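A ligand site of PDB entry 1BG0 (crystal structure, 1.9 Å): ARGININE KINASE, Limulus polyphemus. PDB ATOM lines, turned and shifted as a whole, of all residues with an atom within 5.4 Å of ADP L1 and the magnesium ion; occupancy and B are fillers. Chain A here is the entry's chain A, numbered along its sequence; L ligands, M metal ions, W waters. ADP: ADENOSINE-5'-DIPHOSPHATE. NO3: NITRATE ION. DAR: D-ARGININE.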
ATOM      1  N   SER A 121     -18.743   0.540  28.701  1.00  0.00           N
ATOM      2  CA  SER A 121     -18.735   1.939  29.117  1.00  0.00           C
ATOM      3  C   SER A 121     -19.961   2.698  28.626  1.00  0.00           C
ATOM      4  O   SER A 121     -20.529   2.395  27.580  1.00  0.00           O
ATOM      5  CB  SER A 121     -17.452   2.624  28.629  1.00  0.00           C
ATOM      6  OG  SER A 121     -17.280   2.453  27.234  1.00  0.00           O
ATOM      7  N   THR A 122     -20.370   3.700  29.403  1.00  0.00           N
ATOM      8  CA  THR A 122     -21.530   4.528  29.086  1.00  0.00           C
ATOM      9  C   THR A 122     -21.095   5.978  28.882  1.00  0.00           C
ATOM     10  O   THR A 122     -20.260   6.489  29.618  1.00  0.00           O
ATOM     11  CB  THR A 122     -22.586   4.442  30.188  1.00  0.00           C
ATOM     12  OG1 THR A 122     -22.972   3.072  30.375  1.00  0.00           O
ATOM     13  CG2 THR A 122     -23.819   5.255  29.820  1.00  0.00           C
ATOM     14  N   ARG A 123     -21.719   6.646  27.911  1.00  0.00           N
ATOM     15  CA  ARG A 123     -21.348   8.014  27.585  1.00  0.00           C
ATOM     16  C   ARG A 123     -22.525   8.832  27.066  1.00  0.00           C
ATOM     17  O   ARG A 123     -23.390   8.309  26.364  1.00  0.00           O
ATOM     18  CB  ARG A 123     -20.236   7.983  26.528  1.00  0.00           C
ATOM     19  CG  ARG A 123     -19.750   9.320  25.964  1.00  0.00           C
ATOM     20  CD  ARG A 123     -18.684   9.029  24.903  1.00  0.00           C
ATOM     21  NE  ARG A 123     -18.031  10.208  24.331  1.00  0.00           N
ATOM     22  CZ  ARG A 123     -18.422  10.818  23.226  1.00  0.00           C
ATOM     23  NH1 ARG A 123     -19.488  10.398  22.562  1.00  0.00           N
ATOM     24  NH2 ARG A 123     -17.691  11.813  22.715  1.00  0.00           N
ATOM     25  N   ARG A 125     -23.277  12.820  25.411  1.00  0.00           N
ATOM     26  CA  ARG A 125     -22.707  14.090  24.973  1.00  0.00           C
ATOM     27  C   ARG A 125     -23.750  15.023  24.398  1.00  0.00           C
ATOM     28  O   ARG A 125     -24.812  14.598  23.943  1.00  0.00           O
ATOM     29  CB  ARG A 125     -21.584  13.876  23.948  1.00  0.00           C
ATOM     30  CG  ARG A 125     -22.001  13.235  22.609  1.00  0.00           C
ATOM     31  CD  ARG A 125     -22.615  14.227  21.622  1.00  0.00           C
ATOM     32  NE  ARG A 125     -22.654  13.640  20.282  1.00  0.00           N
ATOM     33  CZ  ARG A 125     -23.490  13.989  19.302  1.00  0.00           C
ATOM     34  NH1 ARG A 125     -24.390  14.950  19.501  1.00  0.00           N
ATOM     35  NH2 ARG A 125     -23.429  13.376  18.134  1.00  0.00           N
ATOM     36  N   ILE A 181      -7.117   9.411  21.862  1.00  0.00           N
ATOM     37  CA  ILE A 181      -8.055   8.935  20.850  1.00  0.00           C
ATOM     38  C   ILE A 181      -8.308   7.446  21.071  1.00  0.00           C
ATOM     39  O   ILE A 181      -9.463   6.995  21.088  1.00  0.00           O
ATOM     40  CB  ILE A 181      -7.531   9.179  19.429  1.00  0.00           C
ATOM     41  CG1 ILE A 181      -7.441  10.687  19.163  1.00  0.00           C
ATOM     42  CG2 ILE A 181      -8.447   8.519  18.411  1.00  0.00           C
ATOM     43  CD1 ILE A 181      -6.866  11.043  17.809  1.00  0.00           C
ATOM     44  N   HIS A 184     -10.652   6.657  23.624  1.00  0.00           N
ATOM     45  CA  HIS A 184     -12.003   7.135  23.325  1.00  0.00           C
ATOM     46  C   HIS A 184     -12.382   8.473  23.947  1.00  0.00           C
ATOM     47  O   HIS A 184     -13.564   8.804  24.035  1.00  0.00           O
ATOM     48  CB  HIS A 184     -13.035   6.068  23.733  1.00  0.00           C
ATOM     49  CG  HIS A 184     -12.712   4.696  23.231  1.00  0.00           C
ATOM     50  ND1 HIS A 184     -12.584   4.398  21.896  1.00  0.00           N
ATOM     51  CD2 HIS A 184     -12.452   3.548  23.904  1.00  0.00           C
ATOM     52  CE1 HIS A 184     -12.259   3.128  21.757  1.00  0.00           C
ATOM     53  NE2 HIS A 184     -12.170   2.589  22.958  1.00  0.00           N
ATOM     54  N   PHE A 185     -11.378   9.252  24.337  1.00  0.00           N
ATOM     55  CA  PHE A 185     -11.631  10.556  24.962  1.00  0.00           C
ATOM     56  C   PHE A 185     -11.610  11.742  23.992  1.00  0.00           C
ATOM     57  O   PHE A 185     -12.510  12.580  24.004  1.00  0.00           O
ATOM     58  CB  PHE A 185     -10.604  10.822  26.069  1.00  0.00           C
ATOM     59  CG  PHE A 185     -10.683   9.848  27.211  1.00  0.00           C
ATOM     60  CD1 PHE A 185     -11.873   9.648  27.894  1.00  0.00           C
ATOM     61  CD2 PHE A 185      -9.559   9.147  27.624  1.00  0.00           C
ATOM     62  CE1 PHE A 185     -11.944   8.767  28.966  1.00  0.00           C
ATOM     63  CE2 PHE A 185      -9.613   8.268  28.690  1.00  0.00           C
ATOM     64  CZ  PHE A 185     -10.808   8.074  29.361  1.00  0.00           C
ATOM     65  N   LEU A 186     -10.581  11.798  23.151  1.00  0.00           N
ATOM     66  CA  LEU A 186     -10.426  12.893  22.196  1.00  0.00           C
ATOM     67  C   LEU A 186     -10.975  12.594  20.803  1.00  0.00           C
ATOM     68  O   LEU A 186     -10.972  11.447  20.361  1.00  0.00           O
ATOM     69  CB  LEU A 186      -8.936  13.258  22.103  1.00  0.00           C
ATOM     70  CG  LEU A 186      -8.472  14.344  21.138  1.00  0.00           C
ATOM     71  CD1 LEU A 186      -9.058  15.698  21.497  1.00  0.00           C
ATOM     72  CD2 LEU A 186      -6.947  14.404  21.187  1.00  0.00           C
ATOM     73  N   TRP A 220     -14.916  19.040  24.105  1.00  0.00           N
ATOM     74  CA  TRP A 220     -14.173  19.166  22.866  1.00  0.00           C
ATOM     75  C   TRP A 220     -14.288  20.606  22.390  1.00  0.00           C
ATOM     76  O   TRP A 220     -15.393  21.154  22.344  1.00  0.00           O
ATOM     77  CB  TRP A 220     -14.772  18.259  21.787  1.00  0.00           C
ATOM     78  CG  TRP A 220     -14.528  16.800  21.967  1.00  0.00           C
ATOM     79  CD1 TRP A 220     -13.735  16.197  22.901  1.00  0.00           C
ATOM     80  CD2 TRP A 220     -15.061  15.750  21.153  1.00  0.00           C
ATOM     81  NE1 TRP A 220     -13.749  14.843  22.722  1.00  0.00           N
ATOM     82  CE2 TRP A 220     -14.549  14.540  21.655  1.00  0.00           C
ATOM     83  CE3 TRP A 220     -15.917  15.723  20.041  1.00  0.00           C
ATOM     84  CZ2 TRP A 220     -14.874  13.308  21.082  1.00  0.00           C
ATOM     85  CZ3 TRP A 220     -16.225  14.502  19.483  1.00  0.00           C
ATOM     86  CH2 TRP A 220     -15.705  13.308  19.999  1.00  0.00           C
ATOM     87  N   GLU A 223     -14.199  21.176  17.177  1.00  0.00           N
ATOM     88  CA  GLU A 223     -14.150  20.054  16.250  1.00  0.00           C
ATOM     89  C   GLU A 223     -15.328  20.271  15.302  1.00  0.00           C
ATOM     90  O   GLU A 223     -15.429  21.319  14.661  1.00  0.00           O
ATOM     91  CB  GLU A 223     -14.296  18.705  16.967  1.00  0.00           C
ATOM     92  CG  GLU A 223     -13.990  17.515  16.068  1.00  0.00           C
ATOM     93  CD  GLU A 223     -15.046  16.430  16.138  1.00  0.00           C
ATOM     94  OE1 GLU A 223     -16.210  16.752  16.469  1.00  0.00           O
ATOM     95  OE2 GLU A 223     -14.721  15.261  15.845  1.00  0.00           O
ATOM     96  N   GLU A 224     -16.252  19.312  15.264  1.00  0.00           N
ATOM     97  CA  GLU A 224     -17.412  19.442  14.393  1.00  0.00           C
ATOM     98  C   GLU A 224     -18.283  20.619  14.829  1.00  0.00           C
ATOM     99  O   GLU A 224     -18.825  21.351  14.004  1.00  0.00           O
ATOM    100  CB  GLU A 224     -18.236  18.144  14.389  1.00  0.00           C
ATOM    101  CG  GLU A 224     -19.476  18.230  13.517  1.00  0.00           C
ATOM    102  CD  GLU A 224     -20.207  16.915  13.403  1.00  0.00           C
ATOM    103  OE1 GLU A 224     -19.548  15.861  13.387  1.00  0.00           O
ATOM    104  OE2 GLU A 224     -21.453  16.932  13.316  1.00  0.00           O
ATOM    105  N   ARG A 228     -18.501  20.328  22.463  1.00  0.00           N
ATOM    106  CA  ARG A 228     -19.113  19.025  22.641  1.00  0.00           C
ATOM    107  C   ARG A 228     -18.844  18.753  24.121  1.00  0.00           C
ATOM    108  O   ARG A 228     -17.701  18.645  24.542  1.00  0.00           O
ATOM    109  CB  ARG A 228     -18.470  17.961  21.761  1.00  0.00           C
ATOM    110  CG  ARG A 228     -18.881  18.020  20.294  1.00  0.00           C
ATOM    111  CD  ARG A 228     -20.385  17.779  20.104  1.00  0.00           C
ATOM    112  NE  ARG A 228     -20.751  17.762  18.690  1.00  0.00           N
ATOM    113  CZ  ARG A 228     -20.624  16.709  17.888  1.00  0.00           C
ATOM    114  NH1 ARG A 228     -20.135  15.566  18.375  1.00  0.00           N
ATOM    115  NH2 ARG A 228     -20.939  16.794  16.602  1.00  0.00           N
ATOM    116  N   MET A 232     -18.665  10.529  30.678  1.00  0.00           N
ATOM    117  CA  MET A 232     -18.491   9.104  30.404  1.00  0.00           C
ATOM    118  C   MET A 232     -17.698   8.378  31.482  1.00  0.00           C
ATOM    119  O   MET A 232     -16.982   9.006  32.270  1.00  0.00           O
ATOM    120  CB  MET A 232     -17.803   8.912  29.045  1.00  0.00           C
ATOM    121  CG  MET A 232     -16.395   9.508  28.983  1.00  0.00           C
ATOM    122  SD  MET A 232     -15.727   9.608  27.300  1.00  0.00           S
ATOM    123  CE  MET A 232     -15.130   7.958  27.055  1.00  0.00           C
ATOM    124  N   ARG A 279     -26.475  12.556  22.309  1.00  0.00           N
ATOM    125  CA  ARG A 279     -26.160  11.206  21.846  1.00  0.00           C
ATOM    126  C   ARG A 279     -25.715  10.394  23.058  1.00  0.00           C
ATOM    127  O   ARG A 279     -24.584  10.538  23.540  1.00  0.00           O
ATOM    128  CB  ARG A 279     -25.069  11.192  20.773  1.00  0.00           C
ATOM    129  CG  ARG A 279     -24.859   9.781  20.167  1.00  0.00           C
ATOM    130  CD  ARG A 279     -23.989   9.800  18.921  1.00  0.00           C
ATOM    131  NE  ARG A 279     -22.577   9.495  19.175  1.00  0.00           N
ATOM    132  CZ  ARG A 279     -22.107   8.274  19.428  1.00  0.00           C
ATOM    133  NH1 ARG A 279     -22.922   7.231  19.460  1.00  0.00           N
ATOM    134  NH2 ARG A 279     -20.804   8.092  19.612  1.00  0.00           N
ATOM    135  N   SER A 281     -24.801   6.910  24.554  1.00  0.00           N
ATOM    136  CA  SER A 281     -24.356   5.637  24.002  1.00  0.00           C
ATOM    137  C   SER A 281     -23.679   4.721  25.007  1.00  0.00           C
ATOM    138  O   SER A 281     -23.366   5.119  26.130  1.00  0.00           O
ATOM    139  CB  SER A 281     -23.378   5.880  22.859  1.00  0.00           C
ATOM    140  OG  SER A 281     -22.148   6.416  23.360  1.00  0.00           O
ATOM    141  N   VAL A 282     -23.466   3.483  24.569  1.00  0.00           N
ATOM    142  CA  VAL A 282     -22.791   2.487  25.365  1.00  0.00           C
ATOM    143  C   VAL A 282     -21.903   1.681  24.439  1.00  0.00           C
ATOM    144  O   VAL A 282     -22.175   1.561  23.246  1.00  0.00           O
ATOM    145  CB  VAL A 282     -23.781   1.489  26.034  1.00  0.00           C
ATOM    146  CG1 VAL A 282     -24.654   2.194  27.057  1.00  0.00           C
ATOM    147  CG2 VAL A 282     -24.618   0.784  24.975  1.00  0.00           C
ATOM    148  N   HIS A 283     -20.777   1.222  24.978  1.00  0.00           N
ATOM    149  CA  HIS A 283     -19.890   0.358  24.237  1.00  0.00           C
ATOM    150  C   HIS A 283     -20.349  -0.965  24.829  1.00  0.00           C
ATOM    151  O   HIS A 283     -20.271  -1.182  26.040  1.00  0.00           O
ATOM    152  CB  HIS A 283     -18.429   0.663  24.571  1.00  0.00           C
ATOM    153  CG  HIS A 283     -17.809   1.641  23.627  1.00  0.00           C
ATOM    154  ND1 HIS A 283     -16.443   1.750  23.457  1.00  0.00           N
ATOM    155  CD2 HIS A 283     -18.370   2.526  22.767  1.00  0.00           C
ATOM    156  CE1 HIS A 283     -16.189   2.663  22.538  1.00  0.00           C
ATOM    157  NE2 HIS A 283     -17.346   3.149  22.095  1.00  0.00           N
ATOM    158  N   ARG A 308     -22.622   1.998  15.765  1.00  0.00           N
ATOM    159  CA  ARG A 308     -21.359   2.550  15.281  1.00  0.00           C
ATOM    160  C   ARG A 308     -20.197   1.662  15.712  1.00  0.00           C
ATOM    161  O   ARG A 308     -20.362   0.798  16.573  1.00  0.00           O
ATOM    162  CB  ARG A 308     -21.139   3.970  15.806  1.00  0.00           C
ATOM    163  CG  ARG A 308     -22.174   4.981  15.368  1.00  0.00           C
ATOM    164  CD  ARG A 308     -21.832   6.386  15.864  1.00  0.00           C
ATOM    165  NE  ARG A 308     -22.848   7.360  15.493  1.00  0.00           N
ATOM    166  CZ  ARG A 308     -22.684   8.678  15.526  1.00  0.00           C
ATOM    167  NH1 ARG A 308     -21.514   9.191  15.907  1.00  0.00           N
ATOM    168  NH2 ARG A 308     -23.670   9.486  15.162  1.00  0.00           N
ATOM    169  N   GLY A 309     -19.036   1.889  15.115  1.00  0.00           N
ATOM    170  CA  GLY A 309     -17.857   1.115  15.459  1.00  0.00           C
ATOM    171  C   GLY A 309     -17.272   1.498  16.800  1.00  0.00           C
ATOM    172  O   GLY A 309     -17.685   2.485  17.410  1.00  0.00           O
ATOM    173  N   THR A 310     -16.282   0.731  17.258  1.00  0.00           N
ATOM    174  CA  THR A 310     -15.660   0.990  18.547  1.00  0.00           C
ATOM    175  C   THR A 310     -14.955   2.342  18.622  1.00  0.00           C
ATOM    176  O   THR A 310     -14.867   2.948  19.686  1.00  0.00           O
ATOM    177  CB  THR A 310     -14.650  -0.101  18.915  1.00  0.00           C
ATOM    178  OG1 THR A 310     -15.191  -1.377  18.563  1.00  0.00           O
ATOM    179  CG2 THR A 310     -14.359  -0.087  20.412  1.00  0.00           C
ATOM    180  N   ARG A 311     -14.446   2.810  17.488  1.00  0.00           N
ATOM    181  CA  ARG A 311     -13.759   4.097  17.455  1.00  0.00           C
ATOM    182  C   ARG A 311     -14.667   5.223  16.990  1.00  0.00           C
ATOM    183  O   ARG A 311     -14.229   6.341  16.733  1.00  0.00           O
ATOM    184  CB  ARG A 311     -12.500   3.993  16.592  1.00  0.00           C
ATOM    185  CG  ARG A 311     -11.515   2.945  17.078  1.00  0.00           C
ATOM    186  CD  ARG A 311     -10.292   2.811  16.175  1.00  0.00           C
ATOM    187  NE  ARG A 311      -9.370   3.932  16.328  1.00  0.00           N
ATOM    188  CZ  ARG A 311      -8.416   3.990  17.248  1.00  0.00           C
ATOM    189  NH1 ARG A 311      -8.260   2.997  18.112  1.00  0.00           N
ATOM    190  NH2 ARG A 311      -7.608   5.036  17.297  1.00  0.00           N
ATOM    191  N   GLY A 312     -15.965   4.922  16.907  1.00  0.00           N
ATOM    192  CA  GLY A 312     -16.923   5.927  16.490  1.00  0.00           C
ATOM    193  C   GLY A 312     -17.570   5.633  15.154  1.00  0.00           C
ATOM    194  O   GLY A 312     -17.390   4.549  14.594  1.00  0.00           O
ATOM    195  N   GLU A 313     -18.336   6.589  14.643  1.00  0.00           N
ATOM    196  CA  GLU A 313     -19.008   6.423  13.363  1.00  0.00           C
ATOM    197  C   GLU A 313     -18.001   6.169  12.245  1.00  0.00           C
ATOM    198  O   GLU A 313     -16.846   6.574  12.342  1.00  0.00           O
ATOM    199  CB  GLU A 313     -19.842   7.669  13.033  1.00  0.00           C
ATOM    200  CG  GLU A 313     -19.042   8.954  12.999  1.00  0.00           C
ATOM    201  CD  GLU A 313     -19.869  10.130  12.504  1.00  0.00           C
ATOM    202  OE1 GLU A 313     -21.046   9.924  12.123  1.00  0.00           O
ATOM    203  OE2 GLU A 313     -19.337  11.252  12.469  1.00  0.00           O
ATOM    204  N   ASP A 323     -20.835   0.449  19.415  1.00  0.00           N
ATOM    205  CA  ASP A 323     -21.291   1.720  19.954  1.00  0.00           C
ATOM    206  C   ASP A 323     -22.763   1.799  19.558  1.00  0.00           C
ATOM    207  O   ASP A 323     -23.088   1.857  18.383  1.00  0.00           O
ATOM    208  CB  ASP A 323     -20.495   2.857  19.296  1.00  0.00           C
ATOM    209  CG  ASP A 323     -20.995   4.235  19.679  1.00  0.00           C
ATOM    210  OD1 ASP A 323     -22.210   4.381  19.963  1.00  0.00           O
ATOM    211  OD2 ASP A 323     -20.186   5.192  19.676  1.00  0.00           O
HETATM  212  PB  ADP L   1     -19.670  11.866  18.847  1.00  0.00           P
HETATM  213  O1B ADP L   1     -18.931  12.833  17.996  1.00  0.00           O
HETATM  214  O2B ADP L   1     -19.280  12.023  20.268  1.00  0.00           O
HETATM  215  O3B ADP L   1     -21.131  11.998  18.650  1.00  0.00           O
HETATM  216  PA  ADP L   1     -18.270   9.685  17.417  1.00  0.00           P
HETATM  217  O1A ADP L   1     -17.705  10.697  16.489  1.00  0.00           O
HETATM  218  O2A ADP L   1     -18.950   8.564  16.729  1.00  0.00           O
HETATM  219  O3A ADP L   1     -19.318  10.337  18.434  1.00  0.00           O
HETATM  220  O5' ADP L   1     -17.140   9.116  18.401  1.00  0.00           O
HETATM  221  C5' ADP L   1     -16.390  10.038  19.190  1.00  0.00           C
HETATM  222  C4' ADP L   1     -15.660   9.265  20.283  1.00  0.00           C
HETATM  223  O4' ADP L   1     -16.582   8.862  21.305  1.00  0.00           O
HETATM  224  C3' ADP L   1     -15.001   7.989  19.768  1.00  0.00           C
HETATM  225  O3' ADP L   1     -13.662   7.919  20.263  1.00  0.00           O
HETATM  226  C2' ADP L   1     -15.808   6.848  20.360  1.00  0.00           C
HETATM  227  O2' ADP L   1     -14.975   5.689  20.546  1.00  0.00           O
HETATM  228  C1' ADP L   1     -16.277   7.500  21.658  1.00  0.00           C
HETATM  229  N9  ADP L   1     -17.427   6.818  22.316  1.00  0.00           N
HETATM  230  C8  ADP L   1     -18.736   6.880  22.015  1.00  0.00           C
HETATM  231  N7  ADP L   1     -19.468   6.225  22.922  1.00  0.00           N
HETATM  232  C5  ADP L   1     -18.572   5.738  23.781  1.00  0.00           C
HETATM  233  C6  ADP L   1     -18.868   4.984  24.908  1.00  0.00           C
HETATM  234  N6  ADP L   1     -20.111   4.713  25.317  1.00  0.00           N
HETATM  235  N1  ADP L   1     -17.806   4.615  25.647  1.00  0.00           N
HETATM  236  C2  ADP L   1     -16.577   4.994  25.298  1.00  0.00           C
HETATM  237  N3  ADP L   1     -16.289   5.720  24.221  1.00  0.00           N
HETATM  238  C4  ADP L   1     -17.300   6.103  23.422  1.00  0.00           C
HETATM  239  N   NO3 L   2     -21.209  12.697  15.558  1.00  0.00           N
HETATM  240  O1  NO3 L   2     -20.032  11.992  15.477  1.00  0.00           O
HETATM  241  O2  NO3 L   2     -22.413  12.026  15.498  1.00  0.00           O
HETATM  242  O3  NO3 L   2     -21.216  14.071  15.773  1.00  0.00           O
HETATM  243  N   DAR L   3     -21.775  13.737   7.158  1.00  0.00           N
HETATM  244  CA  DAR L   3     -21.644  12.310   7.567  1.00  0.00           C
HETATM  245  CB  DAR L   3     -21.942  12.146   9.059  1.00  0.00           C
HETATM  246  CG  DAR L   3     -23.293  12.692   9.507  1.00  0.00           C
HETATM  247  CD  DAR L   3     -23.612  12.226  10.930  1.00  0.00           C
HETATM  248  NE  DAR L   3     -22.446  12.348  11.794  1.00  0.00           N
HETATM  249  CZ  DAR L   3     -22.008  13.491  12.314  1.00  0.00           C
HETATM  250  NH1 DAR L   3     -22.666  14.620  12.051  1.00  0.00           N
HETATM  251  NH2 DAR L   3     -20.907  13.525  13.036  1.00  0.00           N
HETATM  252  C   DAR L   3     -22.581  11.419   6.759  1.00  0.00           C
HETATM  253  O   DAR L   3     -23.439  11.976   6.044  1.00  0.00           O
HETATM  254  OXT DAR L   3     -22.444  10.182   6.849  1.00  0.00           O
HETATM  255 MG    MG M   1     -18.045  12.736  16.142  1.00  0.00          MG
HETATM  256  O   HOH W   1     -15.365  10.200  14.993  1.00  0.00           O
HETATM  257  O   HOH W   2     -11.734   6.005  19.692  1.00  0.00           O
HETATM  258  O   HOH W   3     -17.692  12.496  14.019  1.00  0.00           O
HETATM  259  O   HOH W   4     -19.065  14.598  20.935  1.00  0.00           O
HETATM  260  O   HOH W   5     -17.574   4.531  19.464  1.00  0.00           O
HETATM  261  O   HOH W   6     -16.153  13.047  16.665  1.00  0.00           O
HETATM  262  O   HOH W   7     -12.404   9.806  18.886  1.00  0.00           O
HETATM  263  O   HOH W   8     -18.256  14.770  15.820  1.00  0.00           O
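The guanidinium group of Arg 125 is in salt-bridge range of an oxygen (O3B) of ADP L1.
The side-chain hydroxyl of Ser 281 is in hydrogen-bond range of a nitrogen (N7) of ADP L1.
ND1 of His 184 lies within hydrogen-bond range of O2' of ADP L1, at 3.0 Å.
O of Ser 121 is in hydrogen-bond range of N6 of ADP L1 (3.3 Å).
OG of Ser 121 is in hydrogen-bond range of N1 of ADP L1 (2.7 Å).
NE2 of His 283 lies close to N3 of ADP L1, at 3.5 Å.
NH1 of Arg 123 lies within salt-bridge range of O2B of ADP L1.
N of Glu 313 lies within hydrogen-bond range of O2A of ADP L1 (2.9 Å).
The side-chain carboxylate (OE1) of Glu 224 lies within salt-bridge range of a nitrogen (NH2) of DAR L3.
The side-chain carboxylate (OE1) of Glu 313 lies within salt-bridge range of a nitrogen (NE) of DAR L3 (2.8 Å).
The backbone carbonyl oxygen (O) of Thr 310 lies within hydrogen-bond range of an oxygen (O2') of ADP L1, 2.9 Å away.
The guanidinium group of Arg 228 lies within salt-bridge range of an oxygen (O3B) of ADP L1 (3.7 Å).
An oxygen (O3B) of ADP L1 is in salt-bridge range of the guanidinium group (NE) of Arg 279.
A nitrogen (N6) of ADP L1 lies within hydrogen-bond range of the backbone carbonyl oxygen (O) of Ser 281 (3.4 Å).
O2A of ADP L1 lies within salt-bridge range of NH1 of Arg 308 (2.8 Å).
Water W8 lies within hydrogen-bond range of the side-chain carboxylate (OE1) of Glu 223, the side-chain carboxylate (OE1) of Glu 224 and the guanidinium group (NH1) of Arg 228.
Water W7 lies within hydrogen-bond range of O of Leu 186 (2.6 Å) and O3' of ADP L1 (2.7 Å).
Water W4 lies within hydrogen-bond range of O2B of ADP L1 (2.7 Å) and NH1 of Arg 228 (2.9 Å).
Water W2 lies within hydrogen-bond range of O3' of ADP L1 (2.8 Å), O of Ile 181 (2.8 Å) and ND1 of His 184 (2.9 Å).
No residue comes within 4 Å of the magnesium ion.
OD2 of Asp 323 sits close to N7 of ADP L1 (3.5 Å).
C of Thr 122 touches N6 of ADP L1 (3.9 Å).
Trp 220 touches ADP L1 (CH2 to C5', 3.4 Å).
Met 232 touches ADP L1.
CA of Val 282 touches N6 of ADP L1, at 3.5 Å.
Arg 311 touches ADP L1 (O to C3', 3.5 Å).
CA of Gly 312 touches O2A of ADP L1 (3.3 Å).
The backbone carbonyl oxygen (O) of Arg 228 lies within hydrogen-bond range of the backbone NH (N) of Trp 220, at 2.8 Å.
The side-chain carboxylate of Asp 323 is in salt-bridge range of the guanidinium group of Arg 279.
O of Ser 121 is in hydrogen-bond range of N of His 283, 2.9 Å away.
The side-chain carboxylate of Glu 224 lies within salt-bridge range of the guanidinium group of Arg 228 (3.3 Å).
The backbone carbonyl oxygen (O) of Thr 310 lies close to a ring nitrogen (NE2) of His 283, at 3.5 Å.
NH1 of Arg 308 lies within salt-bridge range of OE1 of Glu 313 (3.9 Å).
The backbone NH (N) of Arg 279 lies within hydrogen-bond range of the backbone carbonyl oxygen (O) of Arg 125.
A ring nitrogen (ND1) of His 184 lies close to the backbone carbonyl oxygen (O) of Thr 310.
The magnesium ion is bound by water W6 (2.0 Å), O1B of ADP L1 (2.1 Å), water W8 (2.1 Å), O1A of ADP L1 (2.1 Å), water W3 (2.2 Å) and O1 of NO3 L2 (2.2 Å).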
